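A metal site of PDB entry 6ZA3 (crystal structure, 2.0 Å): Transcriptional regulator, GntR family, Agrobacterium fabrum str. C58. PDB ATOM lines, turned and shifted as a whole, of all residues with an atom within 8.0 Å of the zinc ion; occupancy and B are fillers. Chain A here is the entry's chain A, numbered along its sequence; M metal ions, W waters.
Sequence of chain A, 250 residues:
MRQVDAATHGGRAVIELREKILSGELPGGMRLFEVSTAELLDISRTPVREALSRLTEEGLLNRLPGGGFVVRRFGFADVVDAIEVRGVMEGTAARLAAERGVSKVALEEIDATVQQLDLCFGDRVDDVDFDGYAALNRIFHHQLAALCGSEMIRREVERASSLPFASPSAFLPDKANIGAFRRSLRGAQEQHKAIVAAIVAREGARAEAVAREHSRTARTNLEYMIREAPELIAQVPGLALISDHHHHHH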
ATOM      1  N   ARG A  86       6.408  15.573 -27.591  1.00  0.00           N
ATOM      2  CA  ARG A  86       6.680  16.721 -26.725  1.00  0.00           C
ATOM      3  C   ARG A  86       5.575  17.768 -26.832  1.00  0.00           C
ATOM      4  O   ARG A  86       5.151  18.305 -25.807  1.00  0.00           O
ATOM      5  CB  ARG A  86       8.071  17.352 -26.944  1.00  0.00           C
ATOM      6  CG  ARG A  86       8.139  18.722 -26.204  1.00  0.00           C
ATOM      7  CD  ARG A  86       9.320  19.605 -26.408  1.00  0.00           C
ATOM      8  NE  ARG A  86       9.697  19.871 -27.800  1.00  0.00           N
ATOM      9  CZ  ARG A  86       9.456  20.994 -28.464  1.00  0.00           C
ATOM     10  NH1 ARG A  86       8.678  21.940 -27.925  1.00  0.00           N
ATOM     11  NH2 ARG A  86       9.960  21.169 -29.682  1.00  0.00           N
ATOM     12  N   GLU A  90       3.335  19.087 -23.736  1.00  0.00           N
ATOM     13  CA  GLU A  90       3.377  20.518 -23.390  1.00  0.00           C
ATOM     14  C   GLU A  90       1.973  21.124 -23.456  1.00  0.00           C
ATOM     15  O   GLU A  90       1.629  21.941 -22.614  1.00  0.00           O
ATOM     16  CB  GLU A  90       4.366  21.309 -24.282  1.00  0.00           C
ATOM     17  CG  GLU A  90       5.799  20.864 -24.011  1.00  0.00           C
ATOM     18  CD  GLU A  90       6.864  21.800 -24.548  1.00  0.00           C
ATOM     19  OE1 GLU A  90       6.744  22.249 -25.718  1.00  0.00           O
ATOM     20  OE2 GLU A  90       7.823  22.069 -23.806  1.00  0.00           O
ATOM     21  N   LEU A 117      12.096  37.338 -22.480  1.00  0.00           N
ATOM     22  CA  LEU A 117      12.213  36.855 -23.855  1.00  0.00           C
ATOM     23  C   LEU A 117      11.955  37.955 -24.892  1.00  0.00           C
ATOM     24  O   LEU A 117      12.639  37.982 -25.911  1.00  0.00           O
ATOM     25  CB  LEU A 117      11.322  35.634 -24.085  1.00  0.00           C
ATOM     26  CG  LEU A 117      11.920  34.287 -23.610  1.00  0.00           C
ATOM     27  CD1 LEU A 117      10.820  33.266 -23.316  1.00  0.00           C
ATOM     28  CD2 LEU A 117      12.917  33.746 -24.643  1.00  0.00           C
ATOM     29  N   TYR A 133      17.961  33.996 -26.021  1.00  0.00           N
ATOM     30  CA  TYR A 133      16.698  33.363 -26.334  1.00  0.00           C
ATOM     31  C   TYR A 133      16.683  31.891 -25.882  1.00  0.00           C
ATOM     32  O   TYR A 133      15.714  31.460 -25.254  1.00  0.00           O
ATOM     33  CB  TYR A 133      16.347  33.454 -27.831  1.00  0.00           C
ATOM     34  CG  TYR A 133      14.962  32.937 -28.128  1.00  0.00           C
ATOM     35  CD1 TYR A 133      14.744  31.566 -28.326  1.00  0.00           C
ATOM     36  CD2 TYR A 133      13.870  33.783 -28.179  1.00  0.00           C
ATOM     37  CE1 TYR A 133      13.458  31.073 -28.576  1.00  0.00           C
ATOM     38  CE2 TYR A 133      12.582  33.291 -28.396  1.00  0.00           C
ATOM     39  CZ  TYR A 133      12.385  31.937 -28.611  1.00  0.00           C
ATOM     40  OH  TYR A 133      11.122  31.478 -28.829  1.00  0.00           O
ATOM     41  N   LEU A 136      16.563  31.451 -21.954  1.00  0.00           N
ATOM     42  CA  LEU A 136      15.255  31.822 -21.431  1.00  0.00           C
ATOM     43  C   LEU A 136      14.169  30.888 -21.897  1.00  0.00           C
ATOM     44  O   LEU A 136      13.212  30.630 -21.150  1.00  0.00           O
ATOM     45  CB  LEU A 136      14.933  33.279 -21.765  1.00  0.00           C
ATOM     46  CG  LEU A 136      15.740  34.320 -21.008  1.00  0.00           C
ATOM     47  CD1 LEU A 136      15.657  35.685 -21.691  1.00  0.00           C
ATOM     48  CD2 LEU A 136      15.322  34.388 -19.528  1.00  0.00           C
ATOM     49  N   ASN A 137      14.323  30.345 -23.113  1.00  0.00           N
ATOM     50  CA  ASN A 137      13.376  29.390 -23.673  1.00  0.00           C
ATOM     51  C   ASN A 137      13.372  28.108 -22.830  1.00  0.00           C
ATOM     52  O   ASN A 137      12.299  27.617 -22.512  1.00  0.00           O
ATOM     53  CB  ASN A 137      13.698  29.086 -25.118  1.00  0.00           C
ATOM     54  CG  ASN A 137      12.651  28.274 -25.807  1.00  0.00           C
ATOM     55  OD1 ASN A 137      11.480  28.632 -25.820  1.00  0.00           O
ATOM     56  ND2 ASN A 137      13.054  27.162 -26.395  1.00  0.00           N
ATOM     57  N   ARG A 138      14.571  27.617 -22.422  1.00  0.00           N
ATOM     58  CA  ARG A 138      14.668  26.433 -21.557  1.00  0.00           C
ATOM     59  C   ARG A 138      13.911  26.693 -20.240  1.00  0.00           C
ATOM     60  O   ARG A 138      13.160  25.826 -19.806  1.00  0.00           O
ATOM     61  CB  ARG A 138      16.111  26.061 -21.253  1.00  0.00           C
ATOM     62  CG  ARG A 138      16.802  25.341 -22.386  1.00  0.00           C
ATOM     63  CD  ARG A 138      18.203  24.873 -22.030  1.00  0.00           C
ATOM     64  NE  ARG A 138      19.167  25.968 -21.997  1.00  0.00           N
ATOM     65  CZ  ARG A 138      19.809  26.438 -23.060  1.00  0.00           C
ATOM     66  NH1 ARG A 138      20.679  27.430 -22.933  1.00  0.00           N
ATOM     67  NH2 ARG A 138      19.597  25.897 -24.260  1.00  0.00           N
ATOM     68  N   PHE A 140      11.407  28.918 -19.637  1.00  0.00           N
ATOM     69  CA  PHE A 140       9.971  28.987 -19.915  1.00  0.00           C
ATOM     70  C   PHE A 140       9.350  27.591 -19.955  1.00  0.00           C
ATOM     71  O   PHE A 140       8.300  27.370 -19.340  1.00  0.00           O
ATOM     72  CB  PHE A 140       9.679  29.719 -21.236  1.00  0.00           C
ATOM     73  CG  PHE A 140       8.213  29.689 -21.626  1.00  0.00           C
ATOM     74  CD1 PHE A 140       7.707  28.665 -22.428  1.00  0.00           C
ATOM     75  CD2 PHE A 140       7.343  30.700 -21.211  1.00  0.00           C
ATOM     76  CE1 PHE A 140       6.354  28.627 -22.788  1.00  0.00           C
ATOM     77  CE2 PHE A 140       5.983  30.655 -21.568  1.00  0.00           C
ATOM     78  CZ  PHE A 140       5.486  29.597 -22.329  1.00  0.00           C
ATOM     79  N   HIS A 141       9.986  26.657 -20.699  1.00  0.00           N
ATOM     80  CA  HIS A 141       9.449  25.317 -20.878  1.00  0.00           C
ATOM     81  C   HIS A 141       9.517  24.508 -19.595  1.00  0.00           C
ATOM     82  O   HIS A 141       8.583  23.748 -19.361  1.00  0.00           O
ATOM     83  CB  HIS A 141      10.086  24.611 -22.070  1.00  0.00           C
ATOM     84  CG  HIS A 141       9.635  25.217 -23.363  1.00  0.00           C
ATOM     85  ND1 HIS A 141       8.557  24.712 -24.050  1.00  0.00           N
ATOM     86  CD2 HIS A 141      10.107  26.294 -24.029  1.00  0.00           C
ATOM     87  CE1 HIS A 141       8.386  25.507 -25.093  1.00  0.00           C
ATOM     88  NE2 HIS A 141       9.284  26.477 -25.109  1.00  0.00           N
ATOM     89  N   LEU A 144       6.606  25.966 -17.627  1.00  0.00           N
ATOM     90  CA  LEU A 144       5.350  25.489 -18.183  1.00  0.00           C
ATOM     91  C   LEU A 144       5.050  24.071 -17.719  1.00  0.00           C
ATOM     92  O   LEU A 144       3.900  23.776 -17.362  1.00  0.00           O
ATOM     93  CB  LEU A 144       5.355  25.563 -19.724  1.00  0.00           C
ATOM     94  CG  LEU A 144       4.086  25.059 -20.427  1.00  0.00           C
ATOM     95  CD1 LEU A 144       2.838  25.821 -19.908  1.00  0.00           C
ATOM     96  CD2 LEU A 144       4.232  25.154 -21.980  1.00  0.00           C
ATOM     97  N   PRO A 168      12.939  21.566 -26.298  1.00  0.00           N
ATOM     98  CA  PRO A 168      12.427  22.840 -26.838  1.00  0.00           C
ATOM     99  C   PRO A 168      13.546  23.750 -27.389  1.00  0.00           C
ATOM    100  O   PRO A 168      13.273  24.699 -28.107  1.00  0.00           O
ATOM    101  CB  PRO A 168      11.711  23.473 -25.621  1.00  0.00           C
ATOM    102  CG  PRO A 168      11.542  22.394 -24.630  1.00  0.00           C
ATOM    103  CD  PRO A 168      12.697  21.483 -24.831  1.00  0.00           C
ATOM    104  N   SER A 169      14.806  23.384 -27.136  1.00  0.00           N
ATOM    105  CA  SER A 169      16.031  24.056 -27.577  1.00  0.00           C
ATOM    106  C   SER A 169      16.643  23.503 -28.871  1.00  0.00           C
ATOM    107  O   SER A 169      17.610  24.108 -29.371  1.00  0.00           O
ATOM    108  CB  SER A 169      17.114  23.914 -26.504  1.00  0.00           C
ATOM    109  OG  SER A 169      16.701  24.375 -25.238  1.00  0.00           O
ATOM    110  N   LEU A 172      17.199  25.660 -32.718  1.00  0.00           N
ATOM    111  CA  LEU A 172      17.351  27.097 -32.505  1.00  0.00           C
ATOM    112  C   LEU A 172      18.648  27.603 -33.147  1.00  0.00           C
ATOM    113  O   LEU A 172      19.599  26.831 -33.242  1.00  0.00           O
ATOM    114  CB  LEU A 172      17.295  27.463 -30.997  1.00  0.00           C
ATOM    115  CG  LEU A 172      16.033  27.088 -30.180  1.00  0.00           C
ATOM    116  CD1 LEU A 172      16.042  27.794 -28.841  1.00  0.00           C
ATOM    117  CD2 LEU A 172      14.733  27.393 -30.925  1.00  0.00           C
ATOM    118  N   LEU A 185      11.842  32.537 -34.697  1.00  0.00           N
ATOM    119  CA  LEU A 185      11.800  32.900 -33.275  1.00  0.00           C
ATOM    120  C   LEU A 185      10.737  33.924 -32.881  1.00  0.00           C
ATOM    121  O   LEU A 185      10.179  33.808 -31.790  1.00  0.00           O
ATOM    122  CB  LEU A 185      13.176  33.352 -32.757  1.00  0.00           C
ATOM    123  CG  LEU A 185      14.324  32.326 -32.868  1.00  0.00           C
ATOM    124  CD1 LEU A 185      15.557  32.825 -32.156  1.00  0.00           C
ATOM    125  CD2 LEU A 185      13.941  30.981 -32.293  1.00  0.00           C
ATOM    126  N   ALA A 188       7.461  31.999 -32.501  1.00  0.00           N
ATOM    127  CA  ALA A 188       7.546  31.170 -31.307  1.00  0.00           C
ATOM    128  C   ALA A 188       7.334  32.026 -30.028  1.00  0.00           C
ATOM    129  O   ALA A 188       6.645  31.585 -29.120  1.00  0.00           O
ATOM    130  CB  ALA A 188       8.863  30.413 -31.258  1.00  0.00           C
ATOM    131  N   GLN A 189       7.876  33.245 -29.980  1.00  0.00           N
ATOM    132  CA  GLN A 189       7.710  34.172 -28.852  1.00  0.00           C
ATOM    133  C   GLN A 189       6.273  34.684 -28.720  1.00  0.00           C
ATOM    134  O   GLN A 189       5.766  34.784 -27.603  1.00  0.00           O
ATOM    135  CB  GLN A 189       8.731  35.336 -28.913  1.00  0.00           C
ATOM    136  CG  GLN A 189       8.534  36.450 -27.848  1.00  0.00           C
ATOM    137  CD  GLN A 189       8.582  36.034 -26.380  1.00  0.00           C
ATOM    138  OE1 GLN A 189       8.829  34.881 -26.014  1.00  0.00           O
ATOM    139  NE2 GLN A 189       8.355  36.983 -25.497  1.00  0.00           N
ATOM    140  N   GLN A 191       3.725  32.932 -29.502  1.00  0.00           N
ATOM    141  CA  GLN A 191       3.090  31.739 -28.947  1.00  0.00           C
ATOM    142  C   GLN A 191       3.329  31.613 -27.437  1.00  0.00           C
ATOM    143  O   GLN A 191       2.415  31.215 -26.739  1.00  0.00           O
ATOM    144  CB  GLN A 191       3.486  30.483 -29.678  1.00  0.00           C
ATOM    145  CG  GLN A 191       2.941  30.492 -31.117  1.00  0.00           C
ATOM    146  CD  GLN A 191       3.704  29.544 -32.005  1.00  0.00           C
ATOM    147  OE1 GLN A 191       4.799  29.072 -31.655  1.00  0.00           O
ATOM    148  NE2 GLN A 191       3.165  29.272 -33.170  1.00  0.00           N
ATOM    149  N   HIS A 192       4.518  31.966 -26.929  1.00  0.00           N
ATOM    150  CA  HIS A 192       4.806  31.951 -25.490  1.00  0.00           C
ATOM    151  C   HIS A 192       3.800  32.908 -24.797  1.00  0.00           C
ATOM    152  O   HIS A 192       3.226  32.559 -23.773  1.00  0.00           O
ATOM    153  CB  HIS A 192       6.218  32.496 -25.203  1.00  0.00           C
ATOM    154  CG  HIS A 192       7.337  31.566 -25.546  1.00  0.00           C
ATOM    155  ND1 HIS A 192       8.602  32.045 -25.841  1.00  0.00           N
ATOM    156  CD2 HIS A 192       7.337  30.215 -25.645  1.00  0.00           C
ATOM    157  CE1 HIS A 192       9.343  30.970 -26.064  1.00  0.00           C
ATOM    158  NE2 HIS A 192       8.621  29.853 -25.974  1.00  0.00           N
ATOM    159  N   ILE A 195       0.261  31.389 -24.877  1.00  0.00           N
ATOM    160  CA  ILE A 195       0.147  30.292 -23.916  1.00  0.00           C
ATOM    161  C   ILE A 195      -0.179  30.832 -22.520  1.00  0.00           C
ATOM    162  O   ILE A 195      -1.106  30.341 -21.879  1.00  0.00           O
ATOM    163  CB  ILE A 195       1.433  29.395 -23.903  1.00  0.00           C
ATOM    164  CG1 ILE A 195       1.641  28.626 -25.259  1.00  0.00           C
ATOM    165  CG2 ILE A 195       1.428  28.424 -22.708  1.00  0.00           C
ATOM    166  CD1 ILE A 195       3.117  28.136 -25.465  1.00  0.00           C
ATOM    167  N   ALA A 211       0.190  25.706 -27.281  1.00  0.00           N
ATOM    168  CA  ALA A 211       1.387  25.004 -26.803  1.00  0.00           C
ATOM    169  C   ALA A 211       1.762  23.867 -27.720  1.00  0.00           C
ATOM    170  O   ALA A 211       2.935  23.698 -28.025  1.00  0.00           O
ATOM    171  CB  ALA A 211       1.215  24.494 -25.375  1.00  0.00           C
ATOM    172  N   HIS A 214       3.343  25.399 -30.927  1.00  0.00           N
ATOM    173  CA  HIS A 214       4.671  25.880 -30.564  1.00  0.00           C
ATOM    174  C   HIS A 214       5.771  24.817 -30.821  1.00  0.00           C
ATOM    175  O   HIS A 214       6.825  25.170 -31.331  1.00  0.00           O
ATOM    176  CB  HIS A 214       4.636  26.345 -29.113  1.00  0.00           C
ATOM    177  CG  HIS A 214       5.890  27.059 -28.718  1.00  0.00           C
ATOM    178  ND1 HIS A 214       6.223  28.301 -29.237  1.00  0.00           N
ATOM    179  CD2 HIS A 214       6.866  26.650 -27.876  1.00  0.00           C
ATOM    180  CE1 HIS A 214       7.380  28.602 -28.686  1.00  0.00           C
ATOM    181  NE2 HIS A 214       7.802  27.651 -27.868  1.00  0.00           N
ATOM    182  N   SER A 215       5.474  23.518 -30.594  1.00  0.00           N
ATOM    183  CA  SER A 215       6.380  22.377 -30.895  1.00  0.00           C
ATOM    184  C   SER A 215       6.552  22.153 -32.378  1.00  0.00           C
ATOM    185  O   SER A 215       7.550  21.559 -32.790  1.00  0.00           O
ATOM    186  CB  SER A 215       5.863  21.093 -30.257  1.00  0.00           C
ATOM    187  OG  SER A 215       4.868  20.449 -31.044  1.00  0.00           O
ATOM    188  N   THR A 217       7.401  24.392 -34.440  1.00  0.00           N
ATOM    189  CA  THR A 217       8.524  25.255 -34.877  1.00  0.00           C
ATOM    190  C   THR A 217       9.710  24.293 -35.216  1.00  0.00           C
ATOM    191  O   THR A 217      10.229  24.336 -36.334  1.00  0.00           O
ATOM    192  CB  THR A 217       8.938  26.304 -33.775  1.00  0.00           C
ATOM    193  OG1 THR A 217       7.856  27.182 -33.447  1.00  0.00           O
ATOM    194  CG2 THR A 217      10.146  27.165 -34.199  1.00  0.00           C
HETATM  195 ZN    ZN M   1       9.395  27.984 -26.565  1.00  0.00          ZN
HETATM  196  O   HOH W   1      10.729  28.608 -28.854  1.00  0.00           O
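The zinc ion is bound by NE2 of His 214, NE2 of His 141, NE2 of His 192 and OD1 of Asn 137. The zinc ion has four donor atoms within binding distance. Slightly farther from the zinc ion lies water W1 (2.7 Å).
The side-chain carboxylate (OE2) of Glu 90 sits at hydrogen-bond distance from a ring nitrogen (ND1) of His 141, 2.8 Å away. ND2 of Asn 137 sits at hydrogen-bond distance from O of Pro 168, 3.0 Å away. The side-chain amide oxygen of Gln 189 lies within hydrogen-bond range of a ring nitrogen (ND1) of His 192 (2.9 Å). A ring nitrogen (ND1) of His 214 sits close to the backbone carbonyl oxygen (O) of Ala 188 (3.3 Å). ND1 of His 214 is in hydrogen-bond range of OE1 of Gln 191, 2.9 Å away. OG1 of Thr 217 sits at hydrogen-bond distance from O of His 214 (3.1 Å).
The nearest printed residue that does not touch the zinc ion is Tyr 133 (4.5 Å).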
